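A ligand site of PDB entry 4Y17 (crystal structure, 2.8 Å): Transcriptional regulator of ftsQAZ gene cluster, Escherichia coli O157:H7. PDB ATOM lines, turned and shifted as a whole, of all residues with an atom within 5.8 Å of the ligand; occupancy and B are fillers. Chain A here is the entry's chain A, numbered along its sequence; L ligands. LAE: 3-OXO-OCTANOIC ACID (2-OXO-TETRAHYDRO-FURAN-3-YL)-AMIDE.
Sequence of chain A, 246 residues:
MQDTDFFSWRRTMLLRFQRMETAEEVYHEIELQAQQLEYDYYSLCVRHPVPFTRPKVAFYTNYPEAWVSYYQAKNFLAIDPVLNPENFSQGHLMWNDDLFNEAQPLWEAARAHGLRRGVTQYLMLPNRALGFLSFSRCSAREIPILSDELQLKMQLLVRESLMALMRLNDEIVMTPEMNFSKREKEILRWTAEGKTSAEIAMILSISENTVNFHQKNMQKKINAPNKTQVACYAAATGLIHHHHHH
OG1 of Thr 61 sits at hydrogen-bond distance from N of Tyr 63.
The backbone carbonyl oxygen of Cys 45 sits at hydrogen-bond distance from the backbone NH of Phe 132, 2.6 Å away.
OD2 of Asp 80 sits at hydrogen-bond distance from OH of Tyr 71 (2.6 Å).
The backbone carbonyl oxygen (O) of Ser 134 sits at hydrogen-bond distance from the backbone NH (N) of Ser 43 (2.8 Å).
OD1 of Asp 80 sits at hydrogen-bond distance from N of Val 82.
N11 of the ligand is in hydrogen-bond range of OD2 of Asp 80.
The side-chain hydroxyl (OG) of Ser 43 lies within hydrogen-bond range of an oxygen (O36) of the ligand.
An oxygen (O10) of the ligand is in hydrogen-bond range of the indole nitrogen of Trp 67, 3.2 Å away.
The side-chain hydroxyl (OH) of Tyr 63 sits close to an oxygen (O10) of the ligand, 3.2 Å away.
Cys 45 touches the ligand (CB to O36, 3.5 Å).
CE1 of Tyr 71 touches C22 of the ligand, 3.6 Å away.
Leu 83 touches the ligand (CD2 to C14, 3.9 Å).
Trp 95 touches the ligand.
Leu 106 touches the ligand.
Ser 134 touches the ligand.
Hydrophobic or aromatic side chains within 4 Å of the ligand: Tyr 63, Trp 67, Tyr 71, Leu 83, Trp 95 and Leu 106.
Of the 21 residues printed, 10 come within 4 Å of the ligand.
Along chain A the residues within 4 Å of the ligand span positions 43 to 134.
The nearest printed residue that does not touch the ligand is Val 82 (4.03 Å).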
ATOM      1  N   SER A  43     -11.833  36.042  -1.400  1.00  0.00           N
ATOM      2  CA  SER A  43     -11.422  35.741  -2.766  1.00  0.00           C
ATOM      3  C   SER A  43     -12.273  36.549  -3.732  1.00  0.00           C
ATOM      4  O   SER A  43     -13.505  36.440  -3.738  1.00  0.00           O
ATOM      5  CB  SER A  43     -11.557  34.253  -3.062  1.00  0.00           C
ATOM      6  OG  SER A  43     -11.198  33.963  -4.391  1.00  0.00           O
ATOM      7  N   LEU A  44     -11.611  37.361  -4.555  1.00  0.00           N
ATOM      8  CA  LEU A  44     -12.294  38.229  -5.499  1.00  0.00           C
ATOM      9  C   LEU A  44     -12.021  37.753  -6.931  1.00  0.00           C
ATOM     10  O   LEU A  44     -10.887  37.831  -7.408  1.00  0.00           O
ATOM     11  CB  LEU A  44     -11.844  39.673  -5.290  1.00  0.00           C
ATOM     12  CG  LEU A  44     -12.570  40.797  -6.027  1.00  0.00           C
ATOM     13  CD1 LEU A  44     -14.067  40.732  -5.779  1.00  0.00           C
ATOM     14  CD2 LEU A  44     -12.027  42.131  -5.550  1.00  0.00           C
ATOM     15  N   CYS A  45     -13.067  37.271  -7.594  1.00  0.00           N
ATOM     16  CA  CYS A  45     -12.945  36.660  -8.912  1.00  0.00           C
ATOM     17  C   CYS A  45     -13.796  37.398  -9.949  1.00  0.00           C
ATOM     18  O   CYS A  45     -14.893  37.857  -9.648  1.00  0.00           O
ATOM     19  CB  CYS A  45     -13.359  35.189  -8.843  1.00  0.00           C
ATOM     20  SG  CYS A  45     -13.163  34.274 -10.390  1.00  0.00           S
ATOM     21  N   PHE A  59      -8.470  36.470 -10.920  1.00  0.00           N
ATOM     22  CA  PHE A  59      -8.847  36.499  -9.504  1.00  0.00           C
ATOM     23  C   PHE A  59      -7.693  36.958  -8.620  1.00  0.00           C
ATOM     24  O   PHE A  59      -6.540  36.991  -9.048  1.00  0.00           O
ATOM     25  CB  PHE A  59      -9.341  35.131  -9.029  1.00  0.00           C
ATOM     26  CG  PHE A  59      -8.293  34.055  -9.068  1.00  0.00           C
ATOM     27  CD1 PHE A  59      -7.345  33.957  -8.064  1.00  0.00           C
ATOM     28  CD2 PHE A  59      -8.275  33.131 -10.102  1.00  0.00           C
ATOM     29  CE1 PHE A  59      -6.378  32.960  -8.090  1.00  0.00           C
ATOM     30  CE2 PHE A  59      -7.314  32.132 -10.135  1.00  0.00           C
ATOM     31  CZ  PHE A  59      -6.365  32.048  -9.136  1.00  0.00           C
ATOM     32  N   THR A  61      -6.736  36.605  -4.236  1.00  0.00           N
ATOM     33  CA  THR A  61      -7.180  36.053  -2.955  1.00  0.00           C
ATOM     34  C   THR A  61      -6.050  35.921  -1.939  1.00  0.00           C
ATOM     35  O   THR A  61      -4.877  35.917  -2.295  1.00  0.00           O
ATOM     36  CB  THR A  61      -7.823  34.658  -3.158  1.00  0.00           C
ATOM     37  OG1 THR A  61      -8.303  34.160  -1.904  1.00  0.00           O
ATOM     38  CG2 THR A  61      -6.799  33.675  -3.734  1.00  0.00           C
ATOM     39  N   TYR A  63      -6.198  33.246   0.014  1.00  0.00           N
ATOM     40  CA  TYR A  63      -6.267  31.817   0.271  1.00  0.00           C
ATOM     41  C   TYR A  63      -4.857  31.253   0.483  1.00  0.00           C
ATOM     42  O   TYR A  63      -3.882  31.836   0.012  1.00  0.00           O
ATOM     43  CB  TYR A  63      -6.945  31.078  -0.887  1.00  0.00           C
ATOM     44  CG  TYR A  63      -8.458  31.015  -0.833  1.00  0.00           C
ATOM     45  CD1 TYR A  63      -9.145  30.932   0.374  1.00  0.00           C
ATOM     46  CD2 TYR A  63      -9.210  31.023  -2.001  1.00  0.00           C
ATOM     47  CE1 TYR A  63     -10.524  30.868   0.417  1.00  0.00           C
ATOM     48  CE2 TYR A  63     -10.589  30.961  -1.972  1.00  0.00           C
ATOM     49  CZ  TYR A  63     -11.246  30.884  -0.763  1.00  0.00           C
ATOM     50  OH  TYR A  63     -12.619  30.825  -0.727  1.00  0.00           O
ATOM     51  N   TRP A  67      -3.787  25.631  -1.393  1.00  0.00           N
ATOM     52  CA  TRP A  67      -5.151  25.435  -1.880  1.00  0.00           C
ATOM     53  C   TRP A  67      -5.360  26.074  -3.253  1.00  0.00           C
ATOM     54  O   TRP A  67      -6.065  25.509  -4.090  1.00  0.00           O
ATOM     55  CB  TRP A  67      -6.150  26.015  -0.876  1.00  0.00           C
ATOM     56  CG  TRP A  67      -7.558  26.045  -1.392  1.00  0.00           C
ATOM     57  CD1 TRP A  67      -8.378  27.137  -1.468  1.00  0.00           C
ATOM     58  CD2 TRP A  67      -8.306  24.952  -1.922  1.00  0.00           C
ATOM     59  NE1 TRP A  67      -9.593  26.791  -2.001  1.00  0.00           N
ATOM     60  CE2 TRP A  67      -9.576  25.451  -2.287  1.00  0.00           C
ATOM     61  CE3 TRP A  67      -8.042  23.591  -2.119  1.00  0.00           C
ATOM     62  CZ2 TRP A  67     -10.565  24.642  -2.839  1.00  0.00           C
ATOM     63  CZ3 TRP A  67      -9.030  22.792  -2.663  1.00  0.00           C
ATOM     64  CH2 TRP A  67     -10.275  23.315  -3.015  1.00  0.00           C
ATOM     65  N   VAL A  68      -4.764  27.234  -3.477  1.00  0.00           N
ATOM     66  CA  VAL A  68      -4.843  27.899  -4.763  1.00  0.00           C
ATOM     67  C   VAL A  68      -4.226  26.998  -5.836  1.00  0.00           C
ATOM     68  O   VAL A  68      -4.821  26.748  -6.885  1.00  0.00           O
ATOM     69  CB  VAL A  68      -4.132  29.264  -4.758  1.00  0.00           C
ATOM     70  CG1 VAL A  68      -4.160  29.906  -6.141  1.00  0.00           C
ATOM     71  CG2 VAL A  68      -4.781  30.190  -3.731  1.00  0.00           C
ATOM     72  N   TYR A  71      -6.425  24.015  -6.495  1.00  0.00           N
ATOM     73  CA  TYR A  71      -7.648  24.432  -7.170  1.00  0.00           C
ATOM     74  C   TYR A  71      -7.415  24.614  -8.664  1.00  0.00           C
ATOM     75  O   TYR A  71      -8.199  24.141  -9.493  1.00  0.00           O
ATOM     76  CB  TYR A  71      -8.152  25.729  -6.551  1.00  0.00           C
ATOM     77  CG  TYR A  71      -9.480  26.221  -7.077  1.00  0.00           C
ATOM     78  CD1 TYR A  71      -9.550  26.996  -8.220  1.00  0.00           C
ATOM     79  CD2 TYR A  71     -10.671  25.901  -6.424  1.00  0.00           C
ATOM     80  CE1 TYR A  71     -10.758  27.456  -8.699  1.00  0.00           C
ATOM     81  CE2 TYR A  71     -11.886  26.357  -6.897  1.00  0.00           C
ATOM     82  CZ  TYR A  71     -11.921  27.129  -8.039  1.00  0.00           C
ATOM     83  OH  TYR A  71     -13.124  27.594  -8.525  1.00  0.00           O
ATOM     84  N   LEU A  77     -12.216  25.971 -11.581  1.00  0.00           N
ATOM     85  CA  LEU A  77     -12.945  27.144 -12.071  1.00  0.00           C
ATOM     86  C   LEU A  77     -14.072  26.720 -12.999  1.00  0.00           C
ATOM     87  O   LEU A  77     -15.136  27.340 -13.027  1.00  0.00           O
ATOM     88  CB  LEU A  77     -12.004  28.108 -12.815  1.00  0.00           C
ATOM     89  CG  LEU A  77     -11.094  29.026 -12.013  1.00  0.00           C
ATOM     90  CD1 LEU A  77     -10.170  29.780 -12.957  1.00  0.00           C
ATOM     91  CD2 LEU A  77     -11.910  30.017 -11.186  1.00  0.00           C
ATOM     92  N   ASP A  80     -16.950  25.195 -10.563  1.00  0.00           N
ATOM     93  CA  ASP A  80     -17.281  25.805  -9.280  1.00  0.00           C
ATOM     94  C   ASP A  80     -18.703  26.376  -9.303  1.00  0.00           C
ATOM     95  O   ASP A  80     -18.989  27.287 -10.086  1.00  0.00           O
ATOM     96  CB  ASP A  80     -16.281  26.917  -8.935  1.00  0.00           C
ATOM     97  CG  ASP A  80     -16.251  27.235  -7.448  1.00  0.00           C
ATOM     98  OD1 ASP A  80     -17.285  27.051  -6.772  1.00  0.00           O
ATOM     99  OD2 ASP A  80     -15.194  27.681  -6.949  1.00  0.00           O
ATOM    100  N   VAL A  82     -20.069  28.130  -7.067  1.00  0.00           N
ATOM    101  CA  VAL A  82     -20.038  29.453  -6.453  1.00  0.00           C
ATOM    102  C   VAL A  82     -19.912  30.542  -7.522  1.00  0.00           C
ATOM    103  O   VAL A  82     -20.294  31.689  -7.304  1.00  0.00           O
ATOM    104  CB  VAL A  82     -18.886  29.568  -5.432  1.00  0.00           C
ATOM    105  CG1 VAL A  82     -18.652  31.009  -5.006  1.00  0.00           C
ATOM    106  CG2 VAL A  82     -19.166  28.712  -4.206  1.00  0.00           C
ATOM    107  N   LEU A  83     -19.389  30.154  -8.680  1.00  0.00           N
ATOM    108  CA  LEU A  83     -19.168  31.085  -9.792  1.00  0.00           C
ATOM    109  C   LEU A  83     -20.266  30.984 -10.845  1.00  0.00           C
ATOM    110  O   LEU A  83     -20.142  31.524 -11.941  1.00  0.00           O
ATOM    111  CB  LEU A  83     -17.807  30.832 -10.429  1.00  0.00           C
ATOM    112  CG  LEU A  83     -16.591  30.944  -9.509  1.00  0.00           C
ATOM    113  CD1 LEU A  83     -15.324  30.533 -10.236  1.00  0.00           C
ATOM    114  CD2 LEU A  83     -16.453  32.351  -8.947  1.00  0.00           C
ATOM    115  N   TRP A  95     -22.840  29.081   1.255  1.00  0.00           N
ATOM    116  CA  TRP A  95     -22.304  27.768   0.900  1.00  0.00           C
ATOM    117  C   TRP A  95     -22.988  26.703   1.746  1.00  0.00           C
ATOM    118  O   TRP A  95     -23.171  26.874   2.948  1.00  0.00           O
ATOM    119  CB  TRP A  95     -20.792  27.705   1.088  1.00  0.00           C
ATOM    120  CG  TRP A  95     -20.019  28.740   0.311  1.00  0.00           C
ATOM    121  CD1 TRP A  95     -20.532  29.701  -0.518  1.00  0.00           C
ATOM    122  CD2 TRP A  95     -18.597  28.889   0.263  1.00  0.00           C
ATOM    123  NE1 TRP A  95     -19.512  30.451  -1.056  1.00  0.00           N
ATOM    124  CE2 TRP A  95     -18.323  29.971  -0.596  1.00  0.00           C
ATOM    125  CE3 TRP A  95     -17.523  28.220   0.865  1.00  0.00           C
ATOM    126  CZ2 TRP A  95     -17.014  30.398  -0.866  1.00  0.00           C
ATOM    127  CZ3 TRP A  95     -16.238  28.644   0.601  1.00  0.00           C
ATOM    128  CH2 TRP A  95     -15.994  29.720  -0.259  1.00  0.00           C
ATOM    129  N   PHE A 100     -22.883  21.598  -3.611  1.00  0.00           N
ATOM    130  CA  PHE A 100     -21.777  20.884  -4.234  1.00  0.00           C
ATOM    131  C   PHE A 100     -22.140  19.438  -4.599  1.00  0.00           C
ATOM    132  O   PHE A 100     -21.258  18.583  -4.714  1.00  0.00           O
ATOM    133  CB  PHE A 100     -20.557  20.916  -3.307  1.00  0.00           C
ATOM    134  CG  PHE A 100     -20.065  22.308  -3.000  1.00  0.00           C
ATOM    135  CD1 PHE A 100     -19.120  22.920  -3.804  1.00  0.00           C
ATOM    136  CD2 PHE A 100     -20.567  23.003  -1.905  1.00  0.00           C
ATOM    137  CE1 PHE A 100     -18.680  24.193  -3.528  1.00  0.00           C
ATOM    138  CE2 PHE A 100     -20.121  24.278  -1.622  1.00  0.00           C
ATOM    139  CZ  PHE A 100     -19.176  24.880  -2.435  1.00  0.00           C
ATOM    140  N   LEU A 106     -14.674  18.992  -5.487  1.00  0.00           N
ATOM    141  CA  LEU A 106     -14.273  20.341  -5.111  1.00  0.00           C
ATOM    142  C   LEU A 106     -14.441  20.516  -3.612  1.00  0.00           C
ATOM    143  O   LEU A 106     -13.540  20.986  -2.910  1.00  0.00           O
ATOM    144  CB  LEU A 106     -15.116  21.384  -5.851  1.00  0.00           C
ATOM    145  CG  LEU A 106     -14.986  22.837  -5.375  1.00  0.00           C
ATOM    146  CD1 LEU A 106     -13.555  23.340  -5.527  1.00  0.00           C
ATOM    147  CD2 LEU A 106     -15.950  23.749  -6.115  1.00  0.00           C
ATOM    148  N   TRP A 107     -15.614  20.130  -3.122  1.00  0.00           N
ATOM    149  CA  TRP A 107     -15.994  20.315  -1.734  1.00  0.00           C
ATOM    150  C   TRP A 107     -15.024  19.607  -0.796  1.00  0.00           C
ATOM    151  O   TRP A 107     -14.544  20.192   0.170  1.00  0.00           O
ATOM    152  CB  TRP A 107     -17.420  19.802  -1.505  1.00  0.00           C
ATOM    153  CG  TRP A 107     -17.977  20.086  -0.138  1.00  0.00           C
ATOM    154  CD1 TRP A 107     -18.497  19.173   0.734  1.00  0.00           C
ATOM    155  CD2 TRP A 107     -18.088  21.367   0.494  1.00  0.00           C
ATOM    156  NE1 TRP A 107     -18.923  19.810   1.876  1.00  0.00           N
ATOM    157  CE2 TRP A 107     -18.682  21.152   1.758  1.00  0.00           C
ATOM    158  CE3 TRP A 107     -17.740  22.664   0.125  1.00  0.00           C
ATOM    159  CZ2 TRP A 107     -18.927  22.190   2.650  1.00  0.00           C
ATOM    160  CZ3 TRP A 107     -17.991  23.700   1.009  1.00  0.00           C
ATOM    161  CH2 TRP A 107     -18.581  23.456   2.253  1.00  0.00           C
ATOM    162  N   ALA A 110     -11.617  21.119  -0.731  1.00  0.00           N
ATOM    163  CA  ALA A 110     -11.673  22.379   0.007  1.00  0.00           C
ATOM    164  C   ALA A 110     -11.693  22.122   1.512  1.00  0.00           C
ATOM    165  O   ALA A 110     -10.984  22.786   2.268  1.00  0.00           O
ATOM    166  CB  ALA A 110     -12.881  23.183  -0.414  1.00  0.00           C
ATOM    167  N   LEU A 115     -11.473  24.574   4.610  1.00  0.00           N
ATOM    168  CA  LEU A 115     -12.591  25.477   4.326  1.00  0.00           C
ATOM    169  C   LEU A 115     -13.939  24.871   4.675  1.00  0.00           C
ATOM    170  O   LEU A 115     -14.548  24.157   3.869  1.00  0.00           O
ATOM    171  CB  LEU A 115     -12.581  25.888   2.849  1.00  0.00           C
ATOM    172  CG  LEU A 115     -11.322  26.596   2.358  1.00  0.00           C
ATOM    173  CD1 LEU A 115     -11.448  26.914   0.882  1.00  0.00           C
ATOM    174  CD2 LEU A 115     -11.087  27.878   3.150  1.00  0.00           C
ATOM    175  N   PHE A 132     -17.219  38.245  -8.568  1.00  0.00           N
ATOM    176  CA  PHE A 132     -17.602  37.393  -7.444  1.00  0.00           C
ATOM    177  C   PHE A 132     -16.702  37.619  -6.235  1.00  0.00           C
ATOM    178  O   PHE A 132     -15.478  37.495  -6.339  1.00  0.00           O
ATOM    179  CB  PHE A 132     -17.538  35.914  -7.856  1.00  0.00           C
ATOM    180  CG  PHE A 132     -18.450  35.550  -8.991  1.00  0.00           C
ATOM    181  CD1 PHE A 132     -19.674  34.955  -8.751  1.00  0.00           C
ATOM    182  CD2 PHE A 132     -18.073  35.797 -10.303  1.00  0.00           C
ATOM    183  CE1 PHE A 132     -20.504  34.612  -9.801  1.00  0.00           C
ATOM    184  CE2 PHE A 132     -18.902  35.455 -11.353  1.00  0.00           C
ATOM    185  CZ  PHE A 132     -20.127  34.857 -11.099  1.00  0.00           C
ATOM    186  N   SER A 134     -16.029  36.097  -2.457  1.00  0.00           N
ATOM    187  CA  SER A 134     -16.282  34.994  -1.544  1.00  0.00           C
ATOM    188  C   SER A 134     -15.538  35.180  -0.231  1.00  0.00           C
ATOM    189  O   SER A 134     -14.363  35.549  -0.227  1.00  0.00           O
ATOM    190  CB  SER A 134     -15.867  33.673  -2.191  1.00  0.00           C
ATOM    191  OG  SER A 134     -16.533  33.459  -3.414  1.00  0.00           O
HETATM  192  C1  LAE L   1     -14.509  28.535  -3.248  1.00  0.00           C
HETATM  193  C2  LAE L   1     -13.236  27.876  -3.021  1.00  0.00           C
HETATM  194  O3  LAE L   1     -13.474  26.419  -3.040  1.00  0.00           O
HETATM  195  C4  LAE L   1     -14.757  26.220  -2.646  1.00  0.00           C
HETATM  196  C5  LAE L   1     -15.528  27.441  -3.027  1.00  0.00           C
HETATM  197  O10 LAE L   1     -12.163  28.425  -2.848  1.00  0.00           O
HETATM  198  N11 LAE L   1     -14.555  28.980  -4.575  1.00  0.00           N
HETATM  199  C13 LAE L   1     -14.074  30.285  -4.868  1.00  0.00           C
HETATM  200  C14 LAE L   1     -14.096  30.798  -6.297  1.00  0.00           C
HETATM  201  C15 LAE L   1     -13.271  32.070  -6.379  1.00  0.00           C
HETATM  202  C18 LAE L   1     -11.862  32.040  -6.922  1.00  0.00           C
HETATM  203  C19 LAE L   1     -11.366  30.615  -6.983  1.00  0.00           C
HETATM  204  C22 LAE L   1      -9.869  30.623  -7.242  1.00  0.00           C
HETATM  205  C25 LAE L   1      -9.144  30.784  -5.920  1.00  0.00           C
HETATM  206  C28 LAE L   1      -8.473  29.472  -5.566  1.00  0.00           C
HETATM  207  O35 LAE L   1     -13.664  30.981  -3.969  1.00  0.00           O
HETATM  208  O36 LAE L   1     -13.749  33.120  -6.009  1.00  0.00           O
